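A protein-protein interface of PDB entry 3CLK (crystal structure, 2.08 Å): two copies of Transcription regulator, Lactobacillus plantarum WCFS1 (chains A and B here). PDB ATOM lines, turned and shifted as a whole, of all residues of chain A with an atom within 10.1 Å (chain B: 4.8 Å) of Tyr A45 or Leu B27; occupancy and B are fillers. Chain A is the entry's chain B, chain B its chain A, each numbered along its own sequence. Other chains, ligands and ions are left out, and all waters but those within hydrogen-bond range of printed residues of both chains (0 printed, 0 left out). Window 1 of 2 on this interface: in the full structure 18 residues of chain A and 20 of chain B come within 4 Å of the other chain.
The backbone NH of Tyr A45 sits at hydrogen-bond distance from the backbone carbonyl oxygen of Leu B41 (3.5 Å). The backbone carbonyl oxygen (O) of Ile B43 is in hydrogen-bond range of the backbone NH (N) of Ile A43, at 2.7 Å.
The backbone NH of Ala A13 lies within hydrogen-bond range of the backbone carbonyl oxygen of Ile A42 (2.9 Å). O of Ala A13 lies within hydrogen-bond range of N of Val A44 (2.9 Å). The backbone NH (N) of Val A15 lies within hydrogen-bond range of the backbone carbonyl oxygen (O) of Val A44, 3.4 Å away.
Ile A42 touches Ile B43 (CA to O, 3.5 Å). Val A44 touches Leu B41 (CA to O, 3.97 Å). Leu B27 touches Tyr A45. OH of Tyr A45 touches OD1 of Asp B28, at 3.9 Å. Tyr A45 touches Gln B31 (CD1 to CG, 3.5 Å). CD2 of Tyr A45 touches CD1 of Ile B43, 3.7 Å away.
Tyr A45 touches five residues of chain B. No residue of chain A comes within 4 Å of Ile B26. Asp B28 touches just one residue of chain A: Tyr A45 (3.9 Å). No residue of chain A comes within 4 Å of Gly B29. No residue of chain A comes within 4 Å of Ile B30. Of chain A, only Tyr A45 (3.5 Å) comes within 4 Å of Gln B31. Of chain A, only Val A44 (3.97 Å) and Tyr A45 (3.5 Å) come within 4 Å of Leu B41. Of the printed residues of chain B, Val A44 touches Leu B41. Of the printed residues of chain B, Ile A43 touches Ile B43. Leu A76 touches none of the printed residues of chain B. The nearest residue of chain A that does not touch Leu B27 is Ile A43 (7.2 Å). The nearest printed residue of chain B that does not touch Val A44 is Ile B43 (4.9 Å).
Of the 13 printed residues of chain B, 5 touch a printed residue of chain A. Along chain B the printed residues that touch a printed residue of chain A span positions 27 to 43. Of the 26 printed residues of chain A, 4 touch a printed residue of chain B. Along chain A the printed residues that touch a printed residue of chain B span positions 42 to 45. Among the printed residues, 8 pairs touch across the chains.
Ile B43 touches its own counterpart, Ile A43. Positions printed for both chains: 13, 23, 27, 43 and 72. Of the 8 pairs that touch across the chains among the printed residues, 1 has its exchanged pair printed and touching as well.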
ATOM      1  N   ALA A  12     -20.670 -17.734   6.295  1.00  0.00           N
ATOM      2  CA  ALA A  12     -21.250 -18.669   5.345  1.00  0.00           C
ATOM      3  C   ALA A  12     -22.725 -18.353   5.170  1.00  0.00           C
ATOM      4  O   ALA A  12     -23.464 -18.233   6.148  1.00  0.00           O
ATOM      5  CB  ALA A  12     -21.075 -20.106   5.844  1.00  0.00           C
ATOM      6  N   ALA A  13     -23.145 -18.204   3.917  1.00  0.00           N
ATOM      7  CA  ALA A  13     -24.534 -17.914   3.607  1.00  0.00           C
ATOM      8  C   ALA A  13     -25.156 -19.147   2.975  1.00  0.00           C
ATOM      9  O   ALA A  13     -24.630 -19.687   2.003  1.00  0.00           O
ATOM     10  CB  ALA A  13     -24.629 -16.730   2.654  1.00  0.00           C
ATOM     11  N   VAL A  14     -26.271 -19.592   3.546  1.00  0.00           N
ATOM     12  CA  VAL A  14     -26.981 -20.760   3.049  1.00  0.00           C
ATOM     13  C   VAL A  14     -28.142 -20.321   2.159  1.00  0.00           C
ATOM     14  O   VAL A  14     -29.011 -19.553   2.581  1.00  0.00           O
ATOM     15  CB  VAL A  14     -27.541 -21.604   4.207  1.00  0.00           C
ATOM     16  CG1 VAL A  14     -28.193 -22.866   3.659  1.00  0.00           C
ATOM     17  CG2 VAL A  14     -26.425 -21.960   5.180  1.00  0.00           C
ATOM     18  N   VAL A  15     -28.140 -20.803   0.923  1.00  0.00           N
ATOM     19  CA  VAL A  15     -29.192 -20.474  -0.030  1.00  0.00           C
ATOM     20  C   VAL A  15     -29.808 -21.760  -0.573  1.00  0.00           C
ATOM     21  O   VAL A  15     -29.123 -22.778  -0.703  1.00  0.00           O
ATOM     22  CB  VAL A  15     -28.637 -19.645  -1.207  1.00  0.00           C
ATOM     23  CG1 VAL A  15     -28.221 -18.266  -0.724  1.00  0.00           C
ATOM     24  CG2 VAL A  15     -27.449 -20.358  -1.827  1.00  0.00           C
ATOM     25  N   SER A  16     -31.103 -21.714  -0.883  1.00  0.00           N
ATOM     26  CA  SER A  16     -31.810 -22.879  -1.405  1.00  0.00           C
ATOM     27  C   SER A  16     -31.219 -23.346  -2.733  1.00  0.00           C
ATOM     28  O   SER A  16     -31.629 -22.894  -3.804  1.00  0.00           O
ATOM     29  CB  SER A  16     -33.292 -22.555  -1.592  1.00  0.00           C
ATOM     30  OG  SER A  16     -33.467 -21.518  -2.542  1.00  0.00           O
ATOM     31  N   ASN A  21     -32.852 -14.256  -7.576  1.00  0.00           N
ATOM     32  CA  ASN A  21     -32.894 -12.819  -7.811  1.00  0.00           C
ATOM     33  C   ASN A  21     -32.980 -12.050  -6.497  1.00  0.00           C
ATOM     34  O   ASN A  21     -32.319 -11.019  -6.326  1.00  0.00           O
ATOM     35  CB  ASN A  21     -34.083 -12.464  -8.705  1.00  0.00           C
ATOM     36  CG  ASN A  21     -35.395 -12.987  -8.162  1.00  0.00           C
ATOM     37  OD1 ASN A  21     -35.566 -14.192  -7.975  1.00  0.00           O
ATOM     38  ND2 ASN A  21     -36.332 -12.081  -7.903  1.00  0.00           N
ATOM     39  N   ALA A  23     -32.133 -13.409  -3.693  1.00  0.00           N
ATOM     40  CA  ALA A  23     -30.946 -13.873  -2.982  1.00  0.00           C
ATOM     41  C   ALA A  23     -29.727 -13.021  -3.323  1.00  0.00           C
ATOM     42  O   ALA A  23     -29.016 -12.564  -2.428  1.00  0.00           O
ATOM     43  CB  ALA A  23     -30.677 -15.331  -3.317  1.00  0.00           C
ATOM     44  N   LEU A  27     -27.279 -11.179  -0.929  1.00  0.00           N
ATOM     45  CA  LEU A  27     -25.854 -11.500  -0.978  1.00  0.00           C
ATOM     46  C   LEU A  27     -24.991 -10.267  -1.236  1.00  0.00           C
ATOM     47  O   LEU A  27     -23.894 -10.154  -0.692  1.00  0.00           O
ATOM     48  CB  LEU A  27     -25.580 -12.562  -2.052  1.00  0.00           C
ATOM     49  CG  LEU A  27     -26.115 -13.979  -1.792  1.00  0.00           C
ATOM     50  CD1 LEU A  27     -25.905 -14.845  -3.026  1.00  0.00           C
ATOM     51  CD2 LEU A  27     -25.417 -14.588  -0.589  1.00  0.00           C
ATOM     52  N   ILE A  42     -18.490 -17.363   2.018  1.00  0.00           N
ATOM     53  CA  ILE A  42     -18.665 -18.562   1.209  1.00  0.00           C
ATOM     54  C   ILE A  42     -20.159 -18.851   1.175  1.00  0.00           C
ATOM     55  O   ILE A  42     -20.870 -18.625   2.158  1.00  0.00           O
ATOM     56  CB  ILE A  42     -17.930 -19.805   1.781  1.00  0.00           C
ATOM     57  CG1 ILE A  42     -18.608 -20.285   3.062  1.00  0.00           C
ATOM     58  CG2 ILE A  42     -16.472 -19.474   2.035  1.00  0.00           C
ATOM     59  CD1 ILE A  42     -18.128 -21.653   3.517  1.00  0.00           C
ATOM     60  N   ILE A  43     -20.634 -19.344   0.040  1.00  0.00           N
ATOM     61  CA  ILE A  43     -22.043 -19.650  -0.124  1.00  0.00           C
ATOM     62  C   ILE A  43     -22.266 -21.155  -0.217  1.00  0.00           C
ATOM     63  O   ILE A  43     -21.803 -21.806  -1.151  1.00  0.00           O
ATOM     64  CB  ILE A  43     -22.597 -18.966  -1.392  1.00  0.00           C
ATOM     65  CG1 ILE A  43     -22.386 -17.452  -1.291  1.00  0.00           C
ATOM     66  CG2 ILE A  43     -24.068 -19.299  -1.566  1.00  0.00           C
ATOM     67  CD1 ILE A  43     -22.755 -16.679  -2.547  1.00  0.00           C
ATOM     68  N   VAL A  44     -22.966 -21.709   0.765  1.00  0.00           N
ATOM     69  CA  VAL A  44     -23.244 -23.137   0.764  1.00  0.00           C
ATOM     70  C   VAL A  44     -24.562 -23.383   0.054  1.00  0.00           C
ATOM     71  O   VAL A  44     -25.632 -23.026   0.553  1.00  0.00           O
ATOM     72  CB  VAL A  44     -23.322 -23.703   2.191  1.00  0.00           C
ATOM     73  CG1 VAL A  44     -23.717 -25.165   2.141  1.00  0.00           C
ATOM     74  CG2 VAL A  44     -21.977 -23.541   2.884  1.00  0.00           C
ATOM     75  N   TYR A  45     -24.470 -24.001  -1.116  1.00  0.00           N
ATOM     76  CA  TYR A  45     -25.631 -24.292  -1.940  1.00  0.00           C
ATOM     77  C   TYR A  45     -26.409 -25.487  -1.408  1.00  0.00           C
ATOM     78  O   TYR A  45     -27.626 -25.417  -1.245  1.00  0.00           O
ATOM     79  CB  TYR A  45     -25.172 -24.546  -3.380  1.00  0.00           C
ATOM     80  CG  TYR A  45     -26.181 -24.151  -4.430  1.00  0.00           C
ATOM     81  CD1 TYR A  45     -27.234 -24.998  -4.771  1.00  0.00           C
ATOM     82  CD2 TYR A  45     -26.086 -22.920  -5.078  1.00  0.00           C
ATOM     83  CE1 TYR A  45     -28.171 -24.631  -5.736  1.00  0.00           C
ATOM     84  CE2 TYR A  45     -27.016 -22.539  -6.042  1.00  0.00           C
ATOM     85  CZ  TYR A  45     -28.056 -23.399  -6.367  1.00  0.00           C
ATOM     86  OH  TYR A  45     -28.975 -23.027  -7.324  1.00  0.00           O
ATOM     87  N   GLU A  52     -31.604 -34.542   2.591  1.00  0.00           N
ATOM     88  CA  GLU A  52     -30.249 -34.508   3.129  1.00  0.00           C
ATOM     89  C   GLU A  52     -29.431 -33.392   2.496  1.00  0.00           C
ATOM     90  O   GLU A  52     -28.404 -32.982   3.037  1.00  0.00           O
ATOM     91  CB  GLU A  52     -29.552 -35.853   2.903  1.00  0.00           C
ATOM     92  CG  GLU A  52     -30.177 -37.003   3.676  1.00  0.00           C
ATOM     93  CD  GLU A  52     -30.127 -36.787   5.176  1.00  0.00           C
ATOM     94  OE1 GLU A  52     -30.625 -35.740   5.646  1.00  0.00           O
ATOM     95  OE2 GLU A  52     -29.590 -37.663   5.887  1.00  0.00           O
ATOM     96  N   GLU A  53     -29.888 -32.909   1.345  1.00  0.00           N
ATOM     97  CA  GLU A  53     -29.206 -31.827   0.648  1.00  0.00           C
ATOM     98  C   GLU A  53     -29.013 -30.713   1.669  1.00  0.00           C
ATOM     99  O   GLU A  53     -28.037 -29.965   1.632  1.00  0.00           O
ATOM    100  CB  GLU A  53     -30.074 -31.320  -0.505  1.00  0.00           C
ATOM    101  CG  GLU A  53     -31.322 -30.563  -0.046  1.00  0.00           C
ATOM    102  CD  GLU A  53     -32.353 -30.381  -1.147  1.00  0.00           C
ATOM    103  OE1 GLU A  53     -33.351 -29.661  -0.913  1.00  0.00           O
ATOM    104  OE2 GLU A  53     -32.171 -30.960  -2.241  1.00  0.00           O
ATOM    105  N   GLN A  54     -29.967 -30.635   2.588  1.00  0.00           N
ATOM    106  CA  GLN A  54     -29.984 -29.636   3.644  1.00  0.00           C
ATOM    107  C   GLN A  54     -28.995 -29.958   4.758  1.00  0.00           C
ATOM    108  O   GLN A  54     -28.060 -29.197   5.013  1.00  0.00           O
ATOM    109  CB  GLN A  54     -31.398 -29.548   4.204  1.00  0.00           C
ATOM    110  CG  GLN A  54     -31.602 -28.522   5.279  1.00  0.00           C
ATOM    111  CD  GLN A  54     -33.068 -28.233   5.495  1.00  0.00           C
ATOM    112  OE1 GLN A  54     -33.739 -27.698   4.612  1.00  0.00           O
ATOM    113  NE2 GLN A  54     -33.582 -28.596   6.664  1.00  0.00           N
ATOM    114  N   LYS A  55     -29.212 -31.087   5.422  1.00  0.00           N
ATOM    115  CA  LYS A  55     -28.348 -31.523   6.510  1.00  0.00           C
ATOM    116  C   LYS A  55     -26.876 -31.394   6.123  1.00  0.00           C
ATOM    117  O   LYS A  55     -26.054 -30.942   6.917  1.00  0.00           O
ATOM    118  CB  LYS A  55     -28.688 -32.971   6.874  1.00  0.00           C
ATOM    119  CG  LYS A  55     -27.996 -33.526   8.110  1.00  0.00           C
ATOM    120  CD  LYS A  55     -26.615 -34.057   7.792  1.00  0.00           C
ATOM    121  CE  LYS A  55     -26.245 -35.167   8.758  1.00  0.00           C
ATOM    122  NZ  LYS A  55     -27.225 -36.289   8.676  1.00  0.00           N
ATOM    123  N   HIS A  56     -26.552 -31.785   4.894  1.00  0.00           N
ATOM    124  CA  HIS A  56     -25.180 -31.711   4.403  1.00  0.00           C
ATOM    125  C   HIS A  56     -24.729 -30.282   4.137  1.00  0.00           C
ATOM    126  O   HIS A  56     -23.534 -29.980   4.165  1.00  0.00           O
ATOM    127  CB  HIS A  56     -25.036 -32.549   3.135  1.00  0.00           C
ATOM    128  CG  HIS A  56     -25.085 -34.022   3.389  1.00  0.00           C
ATOM    129  ND1 HIS A  56     -24.087 -34.691   4.064  1.00  0.00           N
ATOM    130  CD2 HIS A  56     -26.032 -34.946   3.102  1.00  0.00           C
ATOM    131  CE1 HIS A  56     -24.416 -35.964   4.184  1.00  0.00           C
ATOM    132  NE2 HIS A  56     -25.591 -36.146   3.609  1.00  0.00           N
ATOM    133  N   ALA A  57     -25.685 -29.402   3.871  1.00  0.00           N
ATOM    134  CA  ALA A  57     -25.358 -28.009   3.626  1.00  0.00           C
ATOM    135  C   ALA A  57     -24.881 -27.424   4.952  1.00  0.00           C
ATOM    136  O   ALA A  57     -23.855 -26.745   5.007  1.00  0.00           O
ATOM    137  CB  ALA A  57     -26.584 -27.259   3.116  1.00  0.00           C
ATOM    138  N   LEU A  58     -25.628 -27.701   6.019  1.00  0.00           N
ATOM    139  CA  LEU A  58     -25.270 -27.206   7.345  1.00  0.00           C
ATOM    140  C   LEU A  58     -23.891 -27.710   7.744  1.00  0.00           C
ATOM    141  O   LEU A  58     -23.038 -26.933   8.167  1.00  0.00           O
ATOM    142  CB  LEU A  58     -26.288 -27.655   8.399  1.00  0.00           C
ATOM    143  CG  LEU A  58     -27.678 -27.016   8.438  1.00  0.00           C
ATOM    144  CD1 LEU A  58     -27.545 -25.498   8.501  1.00  0.00           C
ATOM    145  CD2 LEU A  58     -28.475 -27.433   7.223  1.00  0.00           C
ATOM    146  N   LEU A  59     -23.671 -29.014   7.609  1.00  0.00           N
ATOM    147  CA  LEU A  59     -22.378 -29.577   7.972  1.00  0.00           C
ATOM    148  C   LEU A  59     -21.265 -29.008   7.112  1.00  0.00           C
ATOM    149  O   LEU A  59     -20.168 -28.763   7.601  1.00  0.00           O
ATOM    150  CB  LEU A  59     -22.389 -31.109   7.867  1.00  0.00           C
ATOM    151  CG  LEU A  59     -23.121 -31.863   8.986  1.00  0.00           C
ATOM    152  CD1 LEU A  59     -22.824 -33.356   8.860  1.00  0.00           C
ATOM    153  CD2 LEU A  59     -22.666 -31.360  10.352  1.00  0.00           C
ATOM    154  N   THR A  60     -21.541 -28.787   5.832  1.00  0.00           N
ATOM    155  CA  THR A  60     -20.523 -28.235   4.948  1.00  0.00           C
ATOM    156  C   THR A  60     -20.060 -26.875   5.458  1.00  0.00           C
ATOM    157  O   THR A  60     -18.902 -26.502   5.281  1.00  0.00           O
ATOM    158  CB  THR A  60     -21.045 -28.060   3.507  1.00  0.00           C
ATOM    159  OG1 THR A  60     -21.418 -29.335   2.969  1.00  0.00           O
ATOM    160  CG2 THR A  60     -19.964 -27.439   2.627  1.00  0.00           C
ATOM    161  N   ALA A  61     -20.968 -26.141   6.096  1.00  0.00           N
ATOM    162  CA  ALA A  61     -20.647 -24.816   6.626  1.00  0.00           C
ATOM    163  C   ALA A  61     -19.980 -24.893   7.998  1.00  0.00           C
ATOM    164  O   ALA A  61     -19.045 -24.142   8.291  1.00  0.00           O
ATOM    165  CB  ALA A  61     -21.913 -23.970   6.712  1.00  0.00           C
ATOM    166  N   LEU A  70     -25.648 -17.294   7.882  1.00  0.00           N
ATOM    167  CA  LEU A  70     -26.844 -16.551   7.512  1.00  0.00           C
ATOM    168  C   LEU A  70     -27.670 -17.461   6.602  1.00  0.00           C
ATOM    169  O   LEU A  70     -27.155 -17.986   5.611  1.00  0.00           O
ATOM    170  CB  LEU A  70     -26.458 -15.271   6.768  1.00  0.00           C
ATOM    171  CG  LEU A  70     -25.596 -14.283   7.563  1.00  0.00           C
ATOM    172  CD1 LEU A  70     -25.183 -13.116   6.667  1.00  0.00           C
ATOM    173  CD2 LEU A  70     -26.384 -13.783   8.762  1.00  0.00           C
ATOM    174  N   LEU A  72     -30.609 -17.627   4.050  1.00  0.00           N
ATOM    175  CA  LEU A  72     -31.477 -16.871   3.164  1.00  0.00           C
ATOM    176  C   LEU A  72     -32.759 -17.602   2.819  1.00  0.00           C
ATOM    177  O   LEU A  72     -32.801 -18.414   1.891  1.00  0.00           O
ATOM    178  CB  LEU A  72     -30.735 -16.519   1.871  1.00  0.00           C
ATOM    179  CG  LEU A  72     -29.408 -15.763   2.002  1.00  0.00           C
ATOM    180  CD1 LEU A  72     -29.065 -15.101   0.668  1.00  0.00           C
ATOM    181  CD2 LEU A  72     -29.518 -14.711   3.084  1.00  0.00           C
ATOM    182  N   ILE A  74     -34.488 -20.108   4.190  1.00  0.00           N
ATOM    183  CA  ILE A  74     -34.396 -21.567   4.158  1.00  0.00           C
ATOM    184  C   ILE A  74     -35.273 -22.137   5.269  1.00  0.00           C
ATOM    185  O   ILE A  74     -35.154 -21.741   6.431  1.00  0.00           O
ATOM    186  CB  ILE A  74     -32.937 -22.069   4.364  1.00  0.00           C
ATOM    187  CG1 ILE A  74     -32.248 -22.278   3.014  1.00  0.00           C
ATOM    188  CG2 ILE A  74     -32.933 -23.387   5.141  1.00  0.00           C
ATOM    189  CD1 ILE A  74     -31.927 -21.013   2.280  1.00  0.00           C
ATOM    190  N   LEU A  76     -35.643 -24.928   7.431  1.00  0.00           N
ATOM    191  CA  LEU A  76     -34.984 -26.113   7.975  1.00  0.00           C
ATOM    192  C   LEU A  76     -35.965 -27.066   8.648  1.00  0.00           C
ATOM    193  O   LEU A  76     -36.965 -26.645   9.217  1.00  0.00           O
ATOM    194  CB  LEU A  76     -33.921 -25.705   8.997  1.00  0.00           C
ATOM    195  CG  LEU A  76     -32.718 -24.896   8.514  1.00  0.00           C
ATOM    196  CD1 LEU A  76     -31.860 -24.514   9.714  1.00  0.00           C
ATOM    197  CD2 LEU A  76     -31.915 -25.707   7.514  1.00  0.00           C
ATOM    198  N   ALA B  13     -16.675 -23.321  -6.212  1.00  0.00           N
ATOM    199  CA  ALA B  13     -17.043 -22.722  -7.483  1.00  0.00           C
ATOM    200  C   ALA B  13     -16.843 -21.225  -7.347  1.00  0.00           C
ATOM    201  O   ALA B  13     -17.467 -20.585  -6.500  1.00  0.00           O
ATOM    202  CB  ALA B  13     -18.497 -23.028  -7.811  1.00  0.00           C
ATOM    203  N   ALA B  23     -24.704 -18.126 -14.394  1.00  0.00           N
ATOM    204  CA  ALA B  23     -24.068 -18.926 -13.350  1.00  0.00           C
ATOM    205  C   ALA B  23     -25.024 -19.957 -12.753  1.00  0.00           C
ATOM    206  O   ALA B  23     -24.680 -21.134 -12.611  1.00  0.00           O
ATOM    207  CB  ALA B  23     -23.523 -18.021 -12.256  1.00  0.00           C
ATOM    208  N   GLN B  24     -26.219 -19.497 -12.402  1.00  0.00           N
ATOM    209  CA  GLN B  24     -27.251 -20.349 -11.830  1.00  0.00           C
ATOM    210  C   GLN B  24     -27.435 -21.599 -12.684  1.00  0.00           C
ATOM    211  O   GLN B  24     -27.576 -22.713 -12.166  1.00  0.00           O
ATOM    212  CB  GLN B  24     -28.568 -19.578 -11.766  1.00  0.00           C
ATOM    213  CG  GLN B  24     -29.802 -20.426 -11.516  1.00  0.00           C
ATOM    214  CD  GLN B  24     -31.089 -19.659 -11.794  1.00  0.00           C
ATOM    215  OE1 GLN B  24     -32.190 -20.213 -11.704  1.00  0.00           O
ATOM    216  NE2 GLN B  24     -30.953 -18.381 -12.136  1.00  0.00           N
ATOM    217  N   GLN B  25     -27.437 -21.399 -13.997  1.00  0.00           N
ATOM    218  CA  GLN B  25     -27.610 -22.490 -14.945  1.00  0.00           C
ATOM    219  C   GLN B  25     -26.479 -23.512 -14.799  1.00  0.00           C
ATOM    220  O   GLN B  25     -26.715 -24.724 -14.788  1.00  0.00           O
ATOM    221  CB  GLN B  25     -27.619 -21.936 -16.370  1.00  0.00           C
ATOM    222  CG  GLN B  25     -28.546 -20.749 -16.593  1.00  0.00           C
ATOM    223  CD  GLN B  25     -30.002 -21.088 -16.352  1.00  0.00           C
ATOM    224  OE1 GLN B  25     -30.511 -22.088 -16.861  1.00  0.00           O
ATOM    225  NE2 GLN B  25     -30.685 -20.250 -15.576  1.00  0.00           N
ATOM    226  N   ILE B  26     -25.252 -23.013 -14.684  1.00  0.00           N
ATOM    227  CA  ILE B  26     -24.081 -23.874 -14.536  1.00  0.00           C
ATOM    228  C   ILE B  26     -24.058 -24.552 -13.167  1.00  0.00           C
ATOM    229  O   ILE B  26     -23.710 -25.728 -13.054  1.00  0.00           O
ATOM    230  CB  ILE B  26     -22.780 -23.066 -14.720  1.00  0.00           C
ATOM    231  CG1 ILE B  26     -22.722 -22.506 -16.144  1.00  0.00           C
ATOM    232  CG2 ILE B  26     -21.564 -23.945 -14.429  1.00  0.00           C
ATOM    233  CD1 ILE B  26     -21.535 -21.600 -16.406  1.00  0.00           C
ATOM    234  N   LEU B  27     -24.432 -23.807 -12.130  1.00  0.00           N
ATOM    235  CA  LEU B  27     -24.451 -24.353 -10.782  1.00  0.00           C
ATOM    236  C   LEU B  27     -25.382 -25.560 -10.701  1.00  0.00           C
ATOM    237  O   LEU B  27     -25.022 -26.585 -10.126  1.00  0.00           O
ATOM    238  CB  LEU B  27     -24.884 -23.281  -9.775  1.00  0.00           C
ATOM    239  CG  LEU B  27     -23.945 -22.081  -9.610  1.00  0.00           C
ATOM    240  CD1 LEU B  27     -24.510 -21.128  -8.567  1.00  0.00           C
ATOM    241  CD2 LEU B  27     -22.564 -22.559  -9.188  1.00  0.00           C
ATOM    242  N   ASP B  28     -26.573 -25.446 -11.287  1.00  0.00           N
ATOM    243  CA  ASP B  28     -27.521 -26.559 -11.273  1.00  0.00           C
ATOM    244  C   ASP B  28     -26.828 -27.834 -11.754  1.00  0.00           C
ATOM    245  O   ASP B  28     -26.984 -28.899 -11.155  1.00  0.00           O
ATOM    246  CB  ASP B  28     -28.733 -26.264 -12.166  1.00  0.00           C
ATOM    247  CG  ASP B  28     -29.598 -25.133 -11.630  1.00  0.00           C
ATOM    248  OD1 ASP B  28     -29.975 -25.168 -10.439  1.00  0.00           O
ATOM    249  OD2 ASP B  28     -29.915 -24.209 -12.407  1.00  0.00           O
ATOM    250  N   GLY B  29     -26.066 -27.719 -12.837  1.00  0.00           N
ATOM    251  CA  GLY B  29     -25.354 -28.869 -13.359  1.00  0.00           C
ATOM    252  C   GLY B  29     -24.356 -29.390 -12.341  1.00  0.00           C
ATOM    253  O   GLY B  29     -24.331 -30.582 -12.035  1.00  0.00           O
ATOM    254  N   ILE B  30     -23.528 -28.493 -11.816  1.00  0.00           N
ATOM    255  CA  ILE B  30     -22.528 -28.853 -10.816  1.00  0.00           C
ATOM    256  C   ILE B  30     -23.192 -29.578  -9.646  1.00  0.00           C
ATOM    257  O   ILE B  30     -22.734 -30.634  -9.219  1.00  0.00           O
ATOM    258  CB  ILE B  30     -21.802 -27.594 -10.289  1.00  0.00           C
ATOM    259  CG1 ILE B  30     -21.012 -26.941 -11.424  1.00  0.00           C
ATOM    260  CG2 ILE B  30     -20.875 -27.960  -9.134  1.00  0.00           C
ATOM    261  CD1 ILE B  30     -20.350 -25.638 -11.044  1.00  0.00           C
ATOM    262  N   GLN B  31     -24.280 -29.009  -9.141  1.00  0.00           N
ATOM    263  CA  GLN B  31     -25.002 -29.604  -8.026  1.00  0.00           C
ATOM    264  C   GLN B  31     -25.397 -31.057  -8.274  1.00  0.00           C
ATOM    265  O   GLN B  31     -25.034 -31.948  -7.504  1.00  0.00           O
ATOM    266  CB  GLN B  31     -26.256 -28.790  -7.711  1.00  0.00           C
ATOM    267  CG  GLN B  31     -26.128 -27.900  -6.487  1.00  0.00           C
ATOM    268  CD  GLN B  31     -25.757 -28.683  -5.235  1.00  0.00           C
ATOM    269  OE1 GLN B  31     -26.445 -29.635  -4.853  1.00  0.00           O
ATOM    270  NE2 GLN B  31     -24.667 -28.281  -4.589  1.00  0.00           N
ATOM    271  N   LEU B  41     -20.865 -28.640  -2.322  1.00  0.00           N
ATOM    272  CA  LEU B  41     -20.560 -27.443  -3.082  1.00  0.00           C
ATOM    273  C   LEU B  41     -20.636 -26.133  -2.309  1.00  0.00           C
ATOM    274  O   LEU B  41     -21.588 -25.879  -1.576  1.00  0.00           O
ATOM    275  CB  LEU B  41     -21.495 -27.377  -4.294  1.00  0.00           C
ATOM    276  CG  LEU B  41     -21.327 -26.232  -5.293  1.00  0.00           C
ATOM    277  CD1 LEU B  41     -19.944 -26.293  -5.927  1.00  0.00           C
ATOM    278  CD2 LEU B  41     -22.414 -26.335  -6.359  1.00  0.00           C
ATOM    279  N   ILE B  43     -19.648 -21.786  -2.829  1.00  0.00           N
ATOM    280  CA  ILE B  43     -19.388 -20.790  -3.851  1.00  0.00           C
ATOM    281  C   ILE B  43     -18.768 -19.525  -3.275  1.00  0.00           C
ATOM    282  O   ILE B  43     -19.123 -19.095  -2.177  1.00  0.00           O
ATOM    283  CB  ILE B  43     -20.700 -20.438  -4.577  1.00  0.00           C
ATOM    284  CG1 ILE B  43     -21.293 -21.706  -5.203  1.00  0.00           C
ATOM    285  CG2 ILE B  43     -20.444 -19.390  -5.634  1.00  0.00           C
ATOM    286  CD1 ILE B  43     -22.707 -21.538  -5.716  1.00  0.00           C
ATOM    287  N   LEU B  72     -16.320 -20.094 -13.000  1.00  0.00           N
ATOM    288  CA  LEU B  72     -17.348 -19.789 -13.984  1.00  0.00           C
ATOM    289  C   LEU B  72     -17.123 -18.410 -14.586  1.00  0.00           C
ATOM    290  O   LEU B  72     -17.397 -17.392 -13.949  1.00  0.00           O
ATOM    291  CB  LEU B  72     -18.739 -19.865 -13.346  1.00  0.00           C
ATOM    292  CG  LEU B  72     -19.079 -21.051 -12.431  1.00  0.00           C
ATOM    293  CD1 LEU B  72     -20.593 -21.167 -12.328  1.00  0.00           C
ATOM    294  CD2 LEU B  72     -18.494 -22.345 -12.963  1.00  0.00           C
